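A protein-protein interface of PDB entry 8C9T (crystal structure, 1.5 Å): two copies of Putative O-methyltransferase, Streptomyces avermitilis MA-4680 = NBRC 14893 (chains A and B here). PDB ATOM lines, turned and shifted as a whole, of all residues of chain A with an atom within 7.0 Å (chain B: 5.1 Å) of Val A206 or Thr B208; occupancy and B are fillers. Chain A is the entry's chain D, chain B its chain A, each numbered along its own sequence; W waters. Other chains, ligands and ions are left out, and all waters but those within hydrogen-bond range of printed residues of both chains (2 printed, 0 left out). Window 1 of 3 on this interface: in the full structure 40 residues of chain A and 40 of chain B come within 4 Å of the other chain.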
ATOM      1  N   VAL A 169     -11.828   0.251  -3.070  1.00  0.00           N
ATOM      2  CA  VAL A 169     -11.988   1.661  -2.620  1.00  0.00           C
ATOM      3  C   VAL A 169     -10.956   2.598  -3.232  1.00  0.00           C
ATOM      4  O   VAL A 169     -10.903   3.794  -2.831  1.00  0.00           O
ATOM      5  CB  VAL A 169     -11.953   1.762  -1.087  1.00  0.00           C
ATOM      6  CG1 VAL A 169     -13.055   0.924  -0.486  1.00  0.00           C
ATOM      7  CG2 VAL A 169     -10.606   1.404  -0.468  1.00  0.00           C
ATOM      8  N   VAL A 170     -10.105   2.104  -4.136  1.00  0.00           N
ATOM      9  CA  VAL A 170      -9.065   2.929  -4.753  1.00  0.00           C
ATOM     10  C   VAL A 170      -9.505   3.491  -6.109  1.00  0.00           C
ATOM     11  O   VAL A 170      -9.067   4.619  -6.376  1.00  0.00           O
ATOM     12  CB  VAL A 170      -7.750   2.107  -4.815  1.00  0.00           C
ATOM     13  CG1 VAL A 170      -6.781   2.735  -5.784  1.00  0.00           C
ATOM     14  CG2 VAL A 170      -7.157   2.055  -3.421  1.00  0.00           C
ATOM     15  N   THR A 204      -9.297   1.943   8.351  1.00  0.00           N
ATOM     16  CA  THR A 204      -8.139   2.259   7.520  1.00  0.00           C
ATOM     17  C   THR A 204      -8.445   1.752   6.125  1.00  0.00           C
ATOM     18  O   THR A 204      -9.434   1.076   5.923  1.00  0.00           O
ATOM     19  CB  THR A 204      -6.842   1.686   8.089  1.00  0.00           C
ATOM     20  OG1 THR A 204      -5.813   2.448   7.441  1.00  0.00           O
ATOM     21  CG2 THR A 204      -6.646   0.214   7.846  1.00  0.00           C
ATOM     22  N   ALA A 205      -7.630   2.149   5.185  1.00  0.00           N
ATOM     23  CA  ALA A 205      -7.677   1.650   3.817  1.00  0.00           C
ATOM     24  C   ALA A 205      -6.255   1.505   3.332  1.00  0.00           C
ATOM     25  O   ALA A 205      -5.387   2.292   3.715  1.00  0.00           O
ATOM     26  CB  ALA A 205      -8.512   2.546   2.912  1.00  0.00           C
ATOM     27  N   VAL A 206      -6.049   0.537   2.462  1.00  0.00           N
ATOM     28  CA  VAL A 206      -4.704   0.211   1.930  1.00  0.00           C
ATOM     29  C   VAL A 206      -4.838  -0.088   0.440  1.00  0.00           C
ATOM     30  O   VAL A 206      -5.828  -0.694   0.035  1.00  0.00           O
ATOM     31  CB  VAL A 206      -4.054  -0.927   2.755  1.00  0.00           C
ATOM     32  CG1 VAL A 206      -2.927  -1.676   2.049  1.00  0.00           C
ATOM     33  CG2 VAL A 206      -3.514  -0.331   4.051  1.00  0.00           C
ATOM     34  N   GLN A 207      -3.806   0.272  -0.310  1.00  0.00           N
ATOM     35  CA  GLN A 207      -3.736  -0.025  -1.754  1.00  0.00           C
ATOM     36  C   GLN A 207      -3.089  -1.378  -1.992  1.00  0.00           C
ATOM     37  O   GLN A 207      -2.073  -1.738  -1.329  1.00  0.00           O
ATOM     38  CB  GLN A 207      -2.881   1.022  -2.457  1.00  0.00           C
ATOM     39  CG  GLN A 207      -3.310   2.445  -2.186  1.00  0.00           C
ATOM     40  CD  GLN A 207      -2.388   3.487  -2.754  1.00  0.00           C
ATOM     41  OE1 GLN A 207      -2.243   3.602  -3.984  1.00  0.00           O
ATOM     42  NE2 GLN A 207      -1.741   4.231  -1.891  1.00  0.00           N
ATOM     43  N   THR A 208      -3.603  -2.066  -2.971  1.00  0.00           N
ATOM     44  CA  THR A 208      -3.097  -3.389  -3.361  1.00  0.00           C
ATOM     45  C   THR A 208      -2.840  -3.403  -4.852  1.00  0.00           C
ATOM     46  O   THR A 208      -3.454  -2.633  -5.617  1.00  0.00           O
ATOM     47  CB  THR A 208      -4.072  -4.501  -2.988  1.00  0.00           C
ATOM     48  OG1 THR A 208      -5.334  -4.289  -3.639  1.00  0.00           O
ATOM     49  CG2 THR A 208      -4.263  -4.598  -1.491  1.00  0.00           C
ATOM     50  N   VAL A 209      -2.005  -4.328  -5.255  1.00  0.00           N
ATOM     51  CA  VAL A 209      -1.863  -4.702  -6.675  1.00  0.00           C
ATOM     52  C   VAL A 209      -1.849  -6.213  -6.757  1.00  0.00           C
ATOM     53  O   VAL A 209      -1.641  -6.901  -5.759  1.00  0.00           O
ATOM     54  CB  VAL A 209      -0.612  -4.093  -7.327  1.00  0.00           C
ATOM     55  CG1 VAL A 209      -0.677  -2.583  -7.387  1.00  0.00           C
ATOM     56  CG2 VAL A 209       0.677  -4.543  -6.645  1.00  0.00           C
ATOM     57  N   ASP A 215      -5.853  -1.637  -6.956  1.00  0.00           N
ATOM     58  CA  ASP A 215      -7.076  -1.248  -6.221  1.00  0.00           C
ATOM     59  C   ASP A 215      -6.725  -1.199  -4.736  1.00  0.00           C
ATOM     60  O   ASP A 215      -5.641  -0.783  -4.400  1.00  0.00           O
ATOM     61  CB  ASP A 215      -8.247  -2.173  -6.507  1.00  0.00           C
ATOM     62  CG  ASP A 215      -9.575  -1.430  -6.530  1.00  0.00           C
ATOM     63  OD1 ASP A 215      -9.757  -0.456  -5.755  1.00  0.00           O
ATOM     64  OD2 ASP A 215     -10.413  -1.775  -7.406  1.00  0.00           O
ATOM     65  N   GLY A 216      -7.679  -1.539  -3.872  1.00  0.00           N
ATOM     66  CA  GLY A 216      -7.421  -1.593  -2.441  1.00  0.00           C
ATOM     67  C   GLY A 216      -8.692  -1.767  -1.689  1.00  0.00           C
ATOM     68  O   GLY A 216      -9.759  -1.863  -2.286  1.00  0.00           O
ATOM     69  N   PHE A 217      -8.587  -1.860  -0.381  1.00  0.00           N
ATOM     70  CA  PHE A 217      -9.738  -2.197   0.459  1.00  0.00           C
ATOM     71  C   PHE A 217      -9.718  -1.336   1.708  1.00  0.00           C
ATOM     72  O   PHE A 217      -8.652  -0.796   2.071  1.00  0.00           O
ATOM     73  CB  PHE A 217      -9.709  -3.693   0.822  1.00  0.00           C
ATOM     74  CG  PHE A 217      -8.550  -4.136   1.663  1.00  0.00           C
ATOM     75  CD1 PHE A 217      -7.361  -4.596   1.126  1.00  0.00           C
ATOM     76  CD2 PHE A 217      -8.675  -4.111   3.039  1.00  0.00           C
ATOM     77  CE1 PHE A 217      -6.274  -4.899   1.936  1.00  0.00           C
ATOM     78  CE2 PHE A 217      -7.605  -4.459   3.851  1.00  0.00           C
ATOM     79  CZ  PHE A 217      -6.417  -4.867   3.302  1.00  0.00           C
ATOM     80  N   ALA A 218     -10.864  -1.223   2.354  1.00  0.00           N
ATOM     81  CA  ALA A 218     -11.018  -0.548   3.658  1.00  0.00           C
ATOM     82  C   ALA A 218     -11.509  -1.558   4.694  1.00  0.00           C
ATOM     83  O   ALA A 218     -12.251  -2.488   4.375  1.00  0.00           O
ATOM     84  CB  ALA A 218     -11.940   0.633   3.606  1.00  0.00           C
ATOM     85  N   LEU A 219     -11.077  -1.378   5.930  1.00  0.00           N
ATOM     86  CA  LEU A 219     -11.522  -2.163   7.101  1.00  0.00           C
ATOM     87  C   LEU A 219     -12.076  -1.178   8.089  1.00  0.00           C
ATOM     88  O   LEU A 219     -11.425  -0.143   8.315  1.00  0.00           O
ATOM     89  CB  LEU A 219     -10.339  -2.856   7.789  1.00  0.00           C
ATOM     90  CG  LEU A 219      -9.579  -3.920   7.062  1.00  0.00           C
ATOM     91  CD1 LEU A 219      -8.682  -4.662   8.068  1.00  0.00           C
ATOM     92  CD2 LEU A 219     -10.540  -4.894   6.421  1.00  0.00           C
ATOM     93  N   PHE B  15      -5.839   8.552   2.361  1.00  0.00           N
ATOM     94  CA  PHE B  15      -6.309   7.541   3.322  1.00  0.00           C
ATOM     95  C   PHE B  15      -5.779   7.862   4.703  1.00  0.00           C
ATOM     96  O   PHE B  15      -6.481   7.700   5.700  1.00  0.00           O
ATOM     97  CB  PHE B  15      -5.824   6.154   2.911  1.00  0.00           C
ATOM     98  CG  PHE B  15      -6.480   5.518   1.713  1.00  0.00           C
ATOM     99  CD1 PHE B  15      -7.711   5.959   1.251  1.00  0.00           C
ATOM    100  CD2 PHE B  15      -5.882   4.445   1.046  1.00  0.00           C
ATOM    101  CE1 PHE B  15      -8.326   5.339   0.175  1.00  0.00           C
ATOM    102  CE2 PHE B  15      -6.505   3.838  -0.016  1.00  0.00           C
ATOM    103  CZ  PHE B  15      -7.757   4.260  -0.418  1.00  0.00           C
ATOM    104  N   ASN B  46      -1.400   4.596   7.319  1.00  0.00           N
ATOM    105  CA  ASN B  46      -2.614   3.778   7.093  1.00  0.00           C
ATOM    106  C   ASN B  46      -2.284   2.288   7.144  1.00  0.00           C
ATOM    107  O   ASN B  46      -3.182   1.515   7.498  1.00  0.00           O
ATOM    108  CB  ASN B  46      -3.306   4.179   5.788  1.00  0.00           C
ATOM    109  CG  ASN B  46      -2.395   4.175   4.589  1.00  0.00           C
ATOM    110  OD1 ASN B  46      -1.269   4.688   4.643  1.00  0.00           O
ATOM    111  ND2 ASN B  46      -2.861   3.600   3.507  1.00  0.00           N
ATOM    112  N   GLN B  47      -1.074   1.829   6.791  1.00  0.00           N
ATOM    113  CA  GLN B  47      -0.637   0.430   7.010  1.00  0.00           C
ATOM    114  C   GLN B  47      -0.327   0.166   8.487  1.00  0.00           C
ATOM    115  O   GLN B  47      -0.624  -0.890   8.990  1.00  0.00           O
ATOM    116  CB  GLN B  47       0.567   0.093   6.125  1.00  0.00           C
ATOM    117  CG  GLN B  47       0.141   0.060   4.672  1.00  0.00           C
ATOM    118  CD  GLN B  47       1.002  -0.816   3.797  1.00  0.00           C
ATOM    119  OE1 GLN B  47       1.454  -1.892   4.195  1.00  0.00           O
ATOM    120  NE2 GLN B  47       1.146  -0.369   2.557  1.00  0.00           N
ATOM    121  N   LEU B  50      -3.579  -0.492   9.935  1.00  0.00           N
ATOM    122  CA  LEU B  50      -3.995  -1.879   9.589  1.00  0.00           C
ATOM    123  C   LEU B  50      -3.369  -2.857  10.592  1.00  0.00           C
ATOM    124  O   LEU B  50      -4.100  -3.690  11.087  1.00  0.00           O
ATOM    125  CB  LEU B  50      -3.586  -2.210   8.158  1.00  0.00           C
ATOM    126  CG  LEU B  50      -3.915  -3.639   7.738  1.00  0.00           C
ATOM    127  CD1 LEU B  50      -5.393  -3.858   7.823  1.00  0.00           C
ATOM    128  CD2 LEU B  50      -3.400  -3.911   6.325  1.00  0.00           C
ATOM    129  N   VAL B 206      -0.080 -10.798   0.267  1.00  0.00           N
ATOM    130  CA  VAL B 206      -0.688  -9.863  -0.707  1.00  0.00           C
ATOM    131  C   VAL B 206       0.325  -8.778  -1.005  1.00  0.00           C
ATOM    132  O   VAL B 206       1.120  -8.400  -0.132  1.00  0.00           O
ATOM    133  CB  VAL B 206      -2.003  -9.270  -0.191  1.00  0.00           C
ATOM    134  CG1 VAL B 206      -3.010 -10.374   0.048  1.00  0.00           C
ATOM    135  CG2 VAL B 206      -1.793  -8.481   1.037  1.00  0.00           C
ATOM    136  N   GLN B 207       0.237  -8.208  -2.191  1.00  0.00           N
ATOM    137  CA  GLN B 207       1.085  -7.098  -2.637  1.00  0.00           C
ATOM    138  C   GLN B 207       0.396  -5.769  -2.370  1.00  0.00           C
ATOM    139  O   GLN B 207      -0.808  -5.647  -2.555  1.00  0.00           O
ATOM    140  CB  GLN B 207       1.286  -7.212  -4.141  1.00  0.00           C
ATOM    141  CG  GLN B 207       1.927  -8.521  -4.616  1.00  0.00           C
ATOM    142  CD  GLN B 207       1.922  -8.632  -6.125  1.00  0.00           C
ATOM    143  OE1 GLN B 207       2.668  -7.923  -6.810  1.00  0.00           O
ATOM    144  NE2 GLN B 207       1.050  -9.474  -6.630  1.00  0.00           N
ATOM    145  N   THR B 208       1.181  -4.846  -1.885  1.00  0.00           N
ATOM    146  CA  THR B 208       0.707  -3.490  -1.560  1.00  0.00           C
ATOM    147  C   THR B 208       1.504  -2.474  -2.351  1.00  0.00           C
ATOM    148  O   THR B 208       2.675  -2.712  -2.688  1.00  0.00           O
ATOM    149  CB  THR B 208       0.773  -3.191  -0.058  1.00  0.00           C
ATOM    150  OG1 THR B 208       2.144  -3.326   0.339  1.00  0.00           O
ATOM    151  CG2 THR B 208      -0.107  -4.088   0.751  1.00  0.00           C
ATOM    152  N   VAL B 209       0.920  -1.307  -2.564  1.00  0.00           N
ATOM    153  CA  VAL B 209       1.657  -0.114  -3.010  1.00  0.00           C
ATOM    154  C   VAL B 209       1.273   1.023  -2.074  1.00  0.00           C
ATOM    155  O   VAL B 209       0.266   0.919  -1.369  1.00  0.00           O
ATOM    156  CB  VAL B 209       1.404   0.208  -4.499  1.00  0.00           C
ATOM    157  CG1 VAL B 209       1.940  -0.882  -5.392  1.00  0.00           C
ATOM    158  CG2 VAL B 209      -0.064   0.490  -4.794  1.00  0.00           C
ATOM    159  N   GLY B 210       2.004   2.103  -2.119  1.00  0.00           N
ATOM    160  CA  GLY B 210       1.720   3.248  -1.256  1.00  0.00           C
ATOM    161  C   GLY B 210       2.988   4.023  -1.044  1.00  0.00           C
ATOM    162  O   GLY B 210       3.934   3.861  -1.849  1.00  0.00           O
ATOM    163  N   GLY B 213       6.358   2.455  -1.271  1.00  0.00           N
ATOM    164  CA  GLY B 213       6.654   1.817  -2.547  1.00  0.00           C
ATOM    165  C   GLY B 213       5.905   0.527  -2.736  1.00  0.00           C
ATOM    166  O   GLY B 213       4.897   0.304  -2.066  1.00  0.00           O
ATOM    167  N   TYR B 214       6.349  -0.295  -3.680  1.00  0.00           N
ATOM    168  CA  TYR B 214       5.799  -1.602  -4.030  1.00  0.00           C
ATOM    169  C   TYR B 214       6.354  -2.639  -3.067  1.00  0.00           C
ATOM    170  O   TYR B 214       7.602  -2.793  -3.001  1.00  0.00           O
ATOM    171  CB  TYR B 214       6.183  -1.893  -5.464  1.00  0.00           C
ATOM    172  CG  TYR B 214       5.891  -3.279  -5.915  1.00  0.00           C
ATOM    173  CD1 TYR B 214       4.646  -3.865  -5.800  1.00  0.00           C
ATOM    174  CD2 TYR B 214       6.849  -4.043  -6.553  1.00  0.00           C
ATOM    175  CE1 TYR B 214       4.401  -5.157  -6.248  1.00  0.00           C
ATOM    176  CE2 TYR B 214       6.608  -5.306  -7.047  1.00  0.00           C
ATOM    177  CZ  TYR B 214       5.390  -5.916  -6.859  1.00  0.00           C
ATOM    178  OH  TYR B 214       5.170  -7.177  -7.313  1.00  0.00           O
ATOM    179  N   ASP B 215       5.489  -3.262  -2.298  1.00  0.00           N
ATOM    180  CA  ASP B 215       5.946  -4.288  -1.344  1.00  0.00           C
ATOM    181  C   ASP B 215       4.793  -5.228  -1.075  1.00  0.00           C
ATOM    182  O   ASP B 215       3.939  -5.380  -1.922  1.00  0.00           O
ATOM    183  CB  ASP B 215       6.464  -3.622  -0.092  1.00  0.00           C
ATOM    184  CG  ASP B 215       7.581  -4.457   0.504  1.00  0.00           C
ATOM    185  OD1 ASP B 215       7.584  -5.709   0.272  1.00  0.00           O
ATOM    186  OD2 ASP B 215       8.484  -3.840   1.111  1.00  0.00           O
ATOM    187  N   GLY B 216       4.755  -5.806   0.118  1.00  0.00           N
ATOM    188  CA  GLY B 216       3.649  -6.683   0.491  1.00  0.00           C
ATOM    189  C   GLY B 216       3.945  -7.372   1.792  1.00  0.00           C
ATOM    190  O   GLY B 216       5.071  -7.249   2.348  1.00  0.00           O
ATOM    191  N   PHE B 217       2.943  -8.080   2.295  1.00  0.00           N
ATOM    192  CA  PHE B 217       3.040  -8.731   3.619  1.00  0.00           C
ATOM    193  C   PHE B 217       2.408 -10.100   3.582  1.00  0.00           C
ATOM    194  O   PHE B 217       1.583 -10.379   2.710  1.00  0.00           O
ATOM    195  CB  PHE B 217       2.384  -7.845   4.678  1.00  0.00           C
ATOM    196  CG  PHE B 217       0.900  -7.703   4.540  1.00  0.00           C
ATOM    197  CD1 PHE B 217       0.057  -8.624   5.121  1.00  0.00           C
ATOM    198  CD2 PHE B 217       0.350  -6.632   3.854  1.00  0.00           C
ATOM    199  CE1 PHE B 217      -1.307  -8.481   5.023  1.00  0.00           C
ATOM    200  CE2 PHE B 217      -1.024  -6.529   3.718  1.00  0.00           C
ATOM    201  CZ  PHE B 217      -1.844  -7.418   4.338  1.00  0.00           C
HETATM  202  O   HOH W   1      -1.794  -9.089  -4.062  1.00  0.00           O
HETATM  203  O   HOH W   2      -1.399   1.549   0.779  1.00  0.00           O
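O of Asn B46 lies within hydrogen-bond range of OG1 of Thr A204.
O of Ala A205 sits at hydrogen-bond distance from ND2 of Asn B46, at 2.9 Å.
The backbone carbonyl oxygen of Gln B207 is in hydrogen-bond range of the backbone NH of Val A209 (3.2 Å).
O of Gln A207 is in hydrogen-bond range of N of Val B209, 3.3 Å away.
The backbone NH of Thr B208 sits at hydrogen-bond distance from the backbone carbonyl oxygen of Asp B215 (2.8 Å).
The side-chain carboxylate of Asp A215 sits at hydrogen-bond distance from the backbone NH of Val A169 (3.5 Å).
The backbone carbonyl oxygen (O) of Gly A216 lies within hydrogen-bond range of the backbone NH (N) of Val A169 (3.1 Å).
The side-chain carboxylate of Asp A215 lies within hydrogen-bond range of the backbone NH of Val A170, 3.0 Å away.
The backbone carbonyl oxygen of Phe A217 is in hydrogen-bond range of the backbone NH of Val A206 (3.0 Å).
The backbone NH (N) of Thr A208 is in hydrogen-bond range of the backbone carbonyl oxygen (O) of Asp A215 (2.8 Å).
Among the printed residues, merely in contact across the chains: Val A169 with Phe B15 (3.99 Å), Val A170 with Phe B15 (3.8 Å), Thr A204 with Leu B50 (3.8 Å), Ala A205 with Phe B15 (3.5 Å), Val A206 with Asn B46 (3.9 Å), Val A206 with Gln B47 (3.7 Å), Val A206 with Thr B208 (3.9 Å), Gln A207 with Thr B208 (3.3 Å), Gln A207 with Gly B210 (3.7 Å), Thr A208 with Gln B207 (3.3 Å), Val A209 with Val B209 (3.7 Å), Val A209 with Tyr B214 (3.8 Å) and Leu A219 with Leu B50 (3.4 Å).
Of the printed residues of chain B, Val A206 touches Asn B46 (3.9 Å), Gln B47 (3.7 Å) and Thr B208 (3.9 Å).
Of the printed residues of chain A, Thr B208 touches Val A206 and Gln A207.
Printed residues of chain A within 4 Å of Val B209: Gln A207 and Val A209.
Printed residues of chain B within 4 Å of Gln A207: Thr B208 (3.3 Å), Val B209 (3.3 Å) and Gly B210 (3.7 Å).
Of the printed residues of chain A, Gln B47 touches Val A206 (3.7 Å).
Of the printed residues of chain B, Ala A205 touches Phe B15 and Asn B46.
Of the printed residues of chain A, Phe B15 touches Val A169 (3.99 Å), Val A170 (3.8 Å) and Ala A205 (3.5 Å).
The nearest printed residue of chain A that does not touch Thr B208 is Thr A208 (4.2 Å).
Of the 14 printed residues of chain B, 9 touch a printed residue of chain A.
Printed residues of chain B that touch a printed residue of chain A: Phe B15, Asn B46, Gln B47, Leu B50, Gln B207, Thr B208, Val B209, Gly B210 and Tyr B214.
Printed residues of chain A that touch a printed residue of chain B: Val A169, Val A170, Thr A204, Ala A205, Val A206, Gln A207, Thr A208, Val A209 and Leu A219.
Hydrophobic or aromatic side chains of chain A within 4 Å of the printed part of chain B: Val A170, Ala A205, Val A206, Val A209 and Leu A219.
Val A206 touches Thr B208, but with the chains exchanged Thr A208 does not touch Val B206 (5.3 Å).
Gln A207 touches Thr B208, and with the chains exchanged Thr A208 touches Gln B207.
Gln A207 touches Val B209, and with the chains exchanged Val A209 touches Gln B207.
Val B209 touches its own counterpart, Val A209.
Of the 17 pairs that touch across the chains among the printed residues, 5 have their exchanged pair printed and touching as well.
Water W1 lies within hydrogen-bond range of O of Val A209 and N of Gln B207.
Water W2 lies within hydrogen-bond range of O of Val B209 (2.8 Å) and N of Gln A207 (2.9 Å).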
